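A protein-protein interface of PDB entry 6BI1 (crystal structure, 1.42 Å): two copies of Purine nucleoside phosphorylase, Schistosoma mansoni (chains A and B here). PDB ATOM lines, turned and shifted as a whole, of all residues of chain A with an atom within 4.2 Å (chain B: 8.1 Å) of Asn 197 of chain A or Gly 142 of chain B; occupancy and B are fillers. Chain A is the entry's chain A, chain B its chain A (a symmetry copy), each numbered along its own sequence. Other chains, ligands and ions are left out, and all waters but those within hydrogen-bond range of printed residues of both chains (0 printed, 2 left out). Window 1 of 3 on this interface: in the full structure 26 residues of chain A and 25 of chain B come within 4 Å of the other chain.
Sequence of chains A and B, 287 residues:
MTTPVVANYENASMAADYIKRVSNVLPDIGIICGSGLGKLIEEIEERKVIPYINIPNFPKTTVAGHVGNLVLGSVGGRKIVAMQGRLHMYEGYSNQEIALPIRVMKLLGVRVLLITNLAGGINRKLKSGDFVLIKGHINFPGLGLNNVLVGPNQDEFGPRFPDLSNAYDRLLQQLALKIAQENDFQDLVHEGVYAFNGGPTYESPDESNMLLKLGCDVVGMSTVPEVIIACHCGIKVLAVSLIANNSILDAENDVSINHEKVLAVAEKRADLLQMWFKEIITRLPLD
Of chain B, only Gly 142 and Leu 143 come within 4 Å of Asn 197 of chain A. Gly 198 of chain A touches just these residues of chain B: Gly 142, Leu 143 and Leu 145. Of chain A, only Asn 197, Gly 198 and Gly 199 come within 4 Å of Gly 142 of chain B. Of the printed residues of chain A, Leu 145 of chain B touches Gly 198 (3.8 Å). Printed residues of chain A within 4 Å of Leu 149 of chain B: Thr 201 (3.8 Å). Of the printed residues of chain A, Val 150 of chain B touches Gly 199. Of the printed residues of chain A, Ile 228 of chain B touches Thr 201. The nearest printed residue of chain A that does not touch Gly 142 of chain B is Thr 201 of chain A (6.0 Å). The nearest printed residue of chain A that does not touch Asn 147 of chain B is Asn 197 of chain A (5.7 Å).
Of the 18 printed residues of chain B, 8 touch a printed residue of chain A. Printed residues of chain B that touch a printed residue of chain A: Gly 142, Leu 143, Leu 145, Asn 147, Leu 149, Val 150, Pro 162 and Ile 228. Hydrophobic or aromatic side chains of chain B that line the printed part of chain A: Leu 143, Leu 145, Leu 149, Val 150, Pro 162 and Ile 228. Among the printed residues, 13 pairs touch across the chains. Among the printed residues, no Asp or Glu carboxylate lies within 4 Å of a Lys or Arg side-chain nitrogen of the other chain.
The backbone carbonyl oxygen (O) of Gly 220 of chain A sits at hydrogen-bond distance from the backbone NH (N) of Asn 197 of chain A. OD1 of Asn 147 of chain B is in hydrogen-bond range of N of Leu 149 of chain B, at 3.0 Å. The side-chain amide nitrogen (ND2) of Asn 197 of chain A lies within hydrogen-bond range of the backbone carbonyl oxygen (O) of Thr 201 of chain A, at 3.1 Å. The side-chain amide oxygen of Asn 139 of chain B lies within hydrogen-bond range of the backbone NH of Gly 142 of chain B. The side-chain amide oxygen of Asn 197 of chain A sits close to the backbone NH of Gly 199 of chain A (3.2 Å).
Among the printed residues, pairs that only touch across the chains: Phe 196 of chain A with Leu 143 of chain B, Asn 197 of chain A with Gly 142 of chain B, Asn 197 of chain A with Leu 143 of chain B, Gly 198 of chain A with Gly 142 of chain B, Gly 198 of chain A with Leu 145 of chain B, Gly 199 of chain A with Gly 142 of chain B, Gly 199 of chain A with Asn 147 of chain B, Gly 199 of chain A with Val 150 of chain B, Thr 201 of chain A with Leu 149 of chain B, Thr 201 of chain A with Pro 162 of chain B and Thr 201 of chain A with Ile 228 of chain B.
Position printed for both chains: 196. Of the 13 pairs that touch across the chains among the printed residues, none has its exchanged pair printed and touching as well.
The side-chain hydroxyl (OG1) of Thr 201 of chain A sits at hydrogen-bond distance from the side-chain amide nitrogen (ND2) of Asn 147 of chain B, at 2.9 Å. The backbone NH of Gly 198 of chain A is in hydrogen-bond range of the backbone carbonyl oxygen of Leu 143 of chain B.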
ATOM      1  N   ALA A 195       8.416 -13.492  -2.177  1.00  0.00           N
ATOM      2  CA  ALA A 195       7.690 -12.358  -2.756  1.00  0.00           C
ATOM      3  C   ALA A 195       7.459 -12.609  -4.246  1.00  0.00           C
ATOM      4  O   ALA A 195       8.409 -12.918  -4.990  1.00  0.00           O
ATOM      5  CB  ALA A 195       8.514 -11.080  -2.619  1.00  0.00           C
ATOM      6  N   PHE A 196       6.206 -12.466  -4.679  1.00  0.00           N
ATOM      7  CA  PHE A 196       5.817 -12.633  -6.082  1.00  0.00           C
ATOM      8  C   PHE A 196       5.875 -11.261  -6.769  1.00  0.00           C
ATOM      9  O   PHE A 196       5.030 -10.395  -6.505  1.00  0.00           O
ATOM     10  CB  PHE A 196       4.418 -13.275  -6.163  1.00  0.00           C
ATOM     11  CG  PHE A 196       3.881 -13.510  -7.575  1.00  0.00           C
ATOM     12  CD1 PHE A 196       4.704 -13.645  -8.683  1.00  0.00           C
ATOM     13  CD2 PHE A 196       2.494 -13.631  -7.785  1.00  0.00           C
ATOM     14  CE1 PHE A 196       4.172 -13.853  -9.973  1.00  0.00           C
ATOM     15  CE2 PHE A 196       1.969 -13.844  -9.039  1.00  0.00           C
ATOM     16  CZ  PHE A 196       2.793 -13.953 -10.153  1.00  0.00           C
ATOM     17  N   ASN A 197       6.903 -11.067  -7.615  1.00  0.00           N
ATOM     18  CA  ASN A 197       7.033  -9.942  -8.561  1.00  0.00           C
ATOM     19  C   ASN A 197       6.424 -10.396  -9.885  1.00  0.00           C
ATOM     20  O   ASN A 197       6.950 -11.312 -10.525  1.00  0.00           O
ATOM     21  CB  ASN A 197       8.530  -9.629  -8.745  1.00  0.00           C
ATOM     22  CG  ASN A 197       8.821  -8.693  -9.919  1.00  0.00           C
ATOM     23  OD1 ASN A 197       7.980  -7.861 -10.309  1.00  0.00           O
ATOM     24  ND2 ASN A 197      10.005  -8.866 -10.525  1.00  0.00           N
ATOM     25  N   GLY A 198       5.329  -9.767 -10.325  1.00  0.00           N
ATOM     26  CA  GLY A 198       4.709 -10.205 -11.577  1.00  0.00           C
ATOM     27  C   GLY A 198       5.652 -10.271 -12.770  1.00  0.00           C
ATOM     28  O   GLY A 198       5.496 -11.138 -13.648  1.00  0.00           O
ATOM     29  N   GLY A 199       6.630  -9.374 -12.844  1.00  0.00           N
ATOM     30  CA  GLY A 199       7.629  -9.419 -13.917  1.00  0.00           C
ATOM     31  C   GLY A 199       7.175  -8.795 -15.241  1.00  0.00           C
ATOM     32  O   GLY A 199       6.074  -8.204 -15.311  1.00  0.00           O
ATOM     33  N   THR A 201      10.512  -7.772 -15.844  1.00  0.00           N
ATOM     34  CA  THR A 201      11.754  -7.130 -15.415  1.00  0.00           C
ATOM     35  C   THR A 201      12.169  -7.665 -14.041  1.00  0.00           C
ATOM     36  O   THR A 201      11.330  -7.851 -13.145  1.00  0.00           O
ATOM     37  CB  THR A 201      11.590  -5.598 -15.345  1.00  0.00           C
ATOM     38  OG1 THR A 201      10.487  -5.253 -14.518  1.00  0.00           O
ATOM     39  CG2 THR A 201      11.350  -4.963 -16.756  1.00  0.00           C
ATOM     40  N   GLU A 203      13.475  -7.383 -10.324  1.00  0.00           N
ATOM     41  CA  GLU A 203      13.304  -6.365  -9.292  1.00  0.00           C
ATOM     42  C   GLU A 203      14.418  -5.330  -9.381  1.00  0.00           C
ATOM     43  O   GLU A 203      15.595  -5.667  -9.545  1.00  0.00           O
ATOM     44  CB  GLU A 203      13.307  -7.055  -7.904  1.00  0.00           C
ATOM     45  CG  GLU A 203      14.675  -7.719  -7.404  1.00  0.00           C
ATOM     46  CD  GLU A 203      14.973  -9.122  -7.931  1.00  0.00           C
ATOM     47  OE1 GLU A 203      16.007  -9.740  -7.522  1.00  0.00           O
ATOM     48  OE2 GLU A 203      14.231  -9.631  -8.768  1.00  0.00           O
ATOM     49  N   VAL A 219      12.685 -13.481  -3.946  1.00  0.00           N
ATOM     50  CA  VAL A 219      11.767 -12.839  -4.895  1.00  0.00           C
ATOM     51  C   VAL A 219      11.819 -13.550  -6.251  1.00  0.00           C
ATOM     52  O   VAL A 219      12.900 -13.873  -6.756  1.00  0.00           O
ATOM     53  CB  VAL A 219      12.022 -11.317  -5.022  1.00  0.00           C
ATOM     54  CG1 VAL A 219      13.446 -10.998  -5.417  1.00  0.00           C
ATOM     55  CG2 VAL A 219      10.986 -10.640  -5.975  1.00  0.00           C
ATOM     56  N   GLY A 220      10.649 -13.827  -6.830  1.00  0.00           N
ATOM     57  CA  GLY A 220      10.608 -14.366  -8.186  1.00  0.00           C
ATOM     58  C   GLY A 220       9.290 -14.095  -8.883  1.00  0.00           C
ATOM     59  O   GLY A 220       8.401 -13.435  -8.331  1.00  0.00           O
ATOM     60  N   MET A 221       9.157 -14.637 -10.105  1.00  0.00           N
ATOM     61  CA  MET A 221       8.069 -14.297 -11.027  1.00  0.00           C
ATOM     62  C   MET A 221       7.095 -15.450 -11.293  1.00  0.00           C
ATOM     63  O   MET A 221       6.374 -15.435 -12.300  1.00  0.00           O
ATOM     64  CB  MET A 221       8.648 -13.789 -12.359  1.00  0.00           C
ATOM     65  CG  MET A 221       9.692 -12.713 -12.252  1.00  0.00           C
ATOM     66  SD  MET A 221      10.387 -12.335 -13.899  1.00  0.00           S
ATOM     67  CE  MET A 221      11.784 -11.354 -13.398  1.00  0.00           C
ATOM     68  N   HIS B 137      13.661   3.542  -8.987  1.00  0.00           N
ATOM     69  CA  HIS B 137      12.198   3.558  -8.865  1.00  0.00           C
ATOM     70  C   HIS B 137      11.639   2.363  -8.092  1.00  0.00           C
ATOM     71  O   HIS B 137      12.287   1.319  -7.940  1.00  0.00           O
ATOM     72  CB  HIS B 137      11.480   3.727 -10.216  1.00  0.00           C
ATOM     73  CG  HIS B 137      11.606   2.558 -11.164  1.00  0.00           C
ATOM     74  ND1 HIS B 137      12.025   2.721 -12.468  1.00  0.00           N
ATOM     75  CD2 HIS B 137      11.293   1.245 -11.027  1.00  0.00           C
ATOM     76  CE1 HIS B 137      11.984   1.553 -13.090  1.00  0.00           C
ATOM     77  NE2 HIS B 137      11.554   0.637 -12.237  1.00  0.00           N
ATOM     78  N   ILE B 138      10.420   2.547  -7.588  1.00  0.00           N
ATOM     79  CA  ILE B 138       9.600   1.460  -7.047  1.00  0.00           C
ATOM     80  C   ILE B 138       8.321   1.392  -7.880  1.00  0.00           C
ATOM     81  O   ILE B 138       7.481   2.313  -7.848  1.00  0.00           O
ATOM     82  CB  ILE B 138       9.306   1.620  -5.546  1.00  0.00           C
ATOM     83  CG1 ILE B 138      10.623   1.502  -4.755  1.00  0.00           C
ATOM     84  CG2 ILE B 138       8.318   0.546  -5.067  1.00  0.00           C
ATOM     85  CD1 ILE B 138      10.516   1.719  -3.291  1.00  0.00           C
ATOM     86  N   ASN B 139       8.168   0.301  -8.640  1.00  0.00           N
ATOM     87  CA  ASN B 139       7.121   0.175  -9.674  1.00  0.00           C
ATOM     88  C   ASN B 139       5.987  -0.689  -9.115  1.00  0.00           C
ATOM     89  O   ASN B 139       5.967  -1.911  -9.320  1.00  0.00           O
ATOM     90  CB  ASN B 139       7.804  -0.491 -10.880  1.00  0.00           C
ATOM     91  CG  ASN B 139       6.904  -0.721 -12.078  1.00  0.00           C
ATOM     92  OD1 ASN B 139       5.768  -0.256 -12.170  1.00  0.00           O
ATOM     93  ND2 ASN B 139       7.454  -1.439 -13.058  1.00  0.00           N
ATOM     94  N   PHE B 140       5.023  -0.071  -8.425  1.00  0.00           N
ATOM     95  CA  PHE B 140       3.928  -0.854  -7.860  1.00  0.00           C
ATOM     96  C   PHE B 140       3.147  -1.590  -8.942  1.00  0.00           C
ATOM     97  O   PHE B 140       2.838  -2.782  -8.737  1.00  0.00           O
ATOM     98  CB  PHE B 140       3.053   0.017  -6.948  1.00  0.00           C
ATOM     99  CG  PHE B 140       3.745   0.424  -5.660  1.00  0.00           C
ATOM    100  CD1 PHE B 140       3.903  -0.486  -4.622  1.00  0.00           C
ATOM    101  CD2 PHE B 140       4.262   1.701  -5.511  1.00  0.00           C
ATOM    102  CE1 PHE B 140       4.568  -0.121  -3.443  1.00  0.00           C
ATOM    103  CE2 PHE B 140       4.924   2.074  -4.347  1.00  0.00           C
ATOM    104  CZ  PHE B 140       5.078   1.160  -3.323  1.00  0.00           C
ATOM    105  N   PRO B 141       2.798  -0.984 -10.075  1.00  0.00           N
ATOM    106  CA  PRO B 141       2.153  -1.781 -11.148  1.00  0.00           C
ATOM    107  C   PRO B 141       2.961  -3.006 -11.565  1.00  0.00           C
ATOM    108  O   PRO B 141       2.383  -4.088 -11.765  1.00  0.00           O
ATOM    109  CB  PRO B 141       1.945  -0.748 -12.281  1.00  0.00           C
ATOM    110  CG  PRO B 141       1.806   0.609 -11.520  1.00  0.00           C
ATOM    111  CD  PRO B 141       2.842   0.466 -10.417  1.00  0.00           C
ATOM    112  N   GLY B 142       4.277  -2.867 -11.717  1.00  0.00           N
ATOM    113  CA  GLY B 142       5.091  -4.002 -12.158  1.00  0.00           C
ATOM    114  C   GLY B 142       5.127  -5.145 -11.154  1.00  0.00           C
ATOM    115  O   GLY B 142       5.006  -6.327 -11.521  1.00  0.00           O
ATOM    116  N   LEU B 143       5.265  -4.826  -9.867  1.00  0.00           N
ATOM    117  CA  LEU B 143       5.191  -5.888  -8.869  1.00  0.00           C
ATOM    118  C   LEU B 143       3.839  -6.594  -8.923  1.00  0.00           C
ATOM    119  O   LEU B 143       3.759  -7.816  -8.696  1.00  0.00           O
ATOM    120  CB  LEU B 143       5.434  -5.312  -7.460  1.00  0.00           C
ATOM    121  CG  LEU B 143       6.861  -4.790  -7.190  1.00  0.00           C
ATOM    122  CD1 LEU B 143       6.882  -4.019  -5.863  1.00  0.00           C
ATOM    123  CD2 LEU B 143       7.916  -5.905  -7.163  1.00  0.00           C
ATOM    124  N   GLY B 144       2.768  -5.836  -9.231  1.00  0.00           N
ATOM    125  CA  GLY B 144       1.396  -6.337  -9.224  1.00  0.00           C
ATOM    126  C   GLY B 144       0.807  -6.892 -10.506  1.00  0.00           C
ATOM    127  O   GLY B 144      -0.432  -6.976 -10.608  1.00  0.00           O
ATOM    128  N   LEU B 145       1.640  -7.315 -11.469  1.00  0.00           N
ATOM    129  CA  LEU B 145       1.235  -7.964 -12.743  1.00  0.00           C
ATOM    130  C   LEU B 145       0.707  -6.991 -13.801  1.00  0.00           C
ATOM    131  O   LEU B 145       0.123  -7.434 -14.819  1.00  0.00           O
ATOM    132  CB  LEU B 145       0.323  -9.206 -12.550  1.00  0.00           C
ATOM    133  CG  LEU B 145       1.028 -10.586 -12.590  1.00  0.00           C
ATOM    134  CD1 LEU B 145       0.007 -11.694 -12.328  1.00  0.00           C
ATOM    135  CD2 LEU B 145       1.735 -10.838 -13.934  1.00  0.00           C
ATOM    136  N   ASN B 146       0.963  -5.680 -13.647  1.00  0.00           N
ATOM    137  CA  ASN B 146       0.643  -4.647 -14.643  1.00  0.00           C
ATOM    138  C   ASN B 146       1.907  -3.960 -15.192  1.00  0.00           C
ATOM    139  O   ASN B 146       1.863  -2.803 -15.626  1.00  0.00           O
ATOM    140  CB  ASN B 146      -0.377  -3.633 -14.102  1.00  0.00           C
ATOM    141  CG  ASN B 146      -1.811  -4.174 -14.066  1.00  0.00           C
ATOM    142  OD1 ASN B 146      -2.178  -5.053 -14.816  1.00  0.00           O
ATOM    143  ND2 ASN B 146      -2.640  -3.617 -13.178  1.00  0.00           N
ATOM    144  N   ASN B 147       3.057  -4.661 -15.211  1.00  0.00           N
ATOM    145  CA  ASN B 147       4.259  -4.138 -15.894  1.00  0.00           C
ATOM    146  C   ASN B 147       3.957  -3.857 -17.367  1.00  0.00           C
ATOM    147  O   ASN B 147       3.235  -4.611 -18.025  1.00  0.00           O
ATOM    148  CB  ASN B 147       5.392  -5.182 -15.743  1.00  0.00           C
ATOM    149  CG  ASN B 147       6.798  -4.643 -16.039  1.00  0.00           C
ATOM    150  OD1 ASN B 147       7.128  -4.241 -17.171  1.00  0.00           O
ATOM    151  ND2 ASN B 147       7.685  -4.732 -15.039  1.00  0.00           N
ATOM    152  N   VAL B 148       4.555  -2.787 -17.898  1.00  0.00           N
ATOM    153  CA  VAL B 148       4.413  -2.447 -19.327  1.00  0.00           C
ATOM    154  C   VAL B 148       4.909  -3.551 -20.271  1.00  0.00           C
ATOM    155  O   VAL B 148       4.500  -3.587 -21.440  1.00  0.00           O
ATOM    156  CB  VAL B 148       5.117  -1.091 -19.590  1.00  0.00           C
ATOM    157  CG1 VAL B 148       6.646  -1.223 -19.495  1.00  0.00           C
ATOM    158  CG2 VAL B 148       4.657  -0.498 -20.941  1.00  0.00           C
ATOM    159  N   LEU B 149       5.783  -4.456 -19.811  1.00  0.00           N
ATOM    160  CA  LEU B 149       6.286  -5.550 -20.646  1.00  0.00           C
ATOM    161  C   LEU B 149       5.484  -6.863 -20.507  1.00  0.00           C
ATOM    162  O   LEU B 149       5.860  -7.862 -21.139  1.00  0.00           O
ATOM    163  CB  LEU B 149       7.801  -5.782 -20.376  1.00  0.00           C
ATOM    164  CG  LEU B 149       8.778  -4.733 -20.926  1.00  0.00           C
ATOM    165  CD1 LEU B 149      10.183  -4.991 -20.406  1.00  0.00           C
ATOM    166  CD2 LEU B 149       8.792  -4.759 -22.462  1.00  0.00           C
ATOM    167  N   VAL B 150       4.410  -6.926 -19.686  1.00  0.00           N
ATOM    168  CA  VAL B 150       3.580  -8.146 -19.656  1.00  0.00           C
ATOM    169  C   VAL B 150       3.004  -8.396 -21.047  1.00  0.00           C
ATOM    170  O   VAL B 150       2.358  -7.514 -21.650  1.00  0.00           O
ATOM    171  CB  VAL B 150       2.467  -8.034 -18.596  1.00  0.00           C
ATOM    172  CG1 VAL B 150       1.457  -9.161 -18.726  1.00  0.00           C
ATOM    173  CG2 VAL B 150       3.047  -8.025 -17.194  1.00  0.00           C
ATOM    174  N   PRO B 162      14.592  -8.030 -18.733  1.00  0.00           N
ATOM    175  CA  PRO B 162      15.557  -6.916 -18.601  1.00  0.00           C
ATOM    176  C   PRO B 162      15.993  -6.643 -17.168  1.00  0.00           C
ATOM    177  O   PRO B 162      15.234  -6.806 -16.204  1.00  0.00           O
ATOM    178  CB  PRO B 162      14.801  -5.698 -19.155  1.00  0.00           C
ATOM    179  CG  PRO B 162      13.581  -6.209 -19.775  1.00  0.00           C
ATOM    180  CD  PRO B 162      13.297  -7.591 -19.311  1.00  0.00           C
ATOM    181  N   PHE B 196       5.957   4.838  -8.475  1.00  0.00           N
ATOM    182  CA  PHE B 196       4.929   4.892  -9.519  1.00  0.00           C
ATOM    183  C   PHE B 196       3.585   4.484  -8.898  1.00  0.00           C
ATOM    184  O   PHE B 196       3.378   3.306  -8.576  1.00  0.00           O
ATOM    185  CB  PHE B 196       5.333   3.985 -10.697  1.00  0.00           C
ATOM    186  CG  PHE B 196       4.348   3.943 -11.866  1.00  0.00           C
ATOM    187  CD1 PHE B 196       3.451   4.967 -12.133  1.00  0.00           C
ATOM    188  CD2 PHE B 196       4.352   2.844 -12.745  1.00  0.00           C
ATOM    189  CE1 PHE B 196       2.550   4.889 -13.217  1.00  0.00           C
ATOM    190  CE2 PHE B 196       3.483   2.767 -13.809  1.00  0.00           C
ATOM    191  CZ  PHE B 196       2.565   3.780 -14.062  1.00  0.00           C
ATOM    192  N   VAL B 224       7.712   5.798 -15.419  1.00  0.00           N
ATOM    193  CA  VAL B 224       8.262   4.437 -15.300  1.00  0.00           C
ATOM    194  C   VAL B 224       7.947   3.555 -16.509  1.00  0.00           C
ATOM    195  O   VAL B 224       8.830   2.791 -16.936  1.00  0.00           O
ATOM    196  CB  VAL B 224       7.892   3.837 -13.938  1.00  0.00           C
ATOM    197  CG1 VAL B 224       8.164   2.345 -13.836  1.00  0.00           C
ATOM    198  CG2 VAL B 224       8.623   4.582 -12.787  1.00  0.00           C
ATOM    199  N   ILE B 228      11.055   1.889 -18.803  1.00  0.00           N
ATOM    200  CA  ILE B 228      11.245   0.451 -18.981  1.00  0.00           C
ATOM    201  C   ILE B 228      11.326   0.081 -20.469  1.00  0.00           C
ATOM    202  O   ILE B 228      12.199  -0.707 -20.882  1.00  0.00           O
ATOM    203  CB  ILE B 228      10.151  -0.327 -18.221  1.00  0.00           C
ATOM    204  CG1 ILE B 228      10.425  -0.241 -16.714  1.00  0.00           C
ATOM    205  CG2 ILE B 228      10.100  -1.833 -18.705  1.00  0.00           C
ATOM    206  CD1 ILE B 228       9.316  -0.795 -15.836  1.00  0.00           C
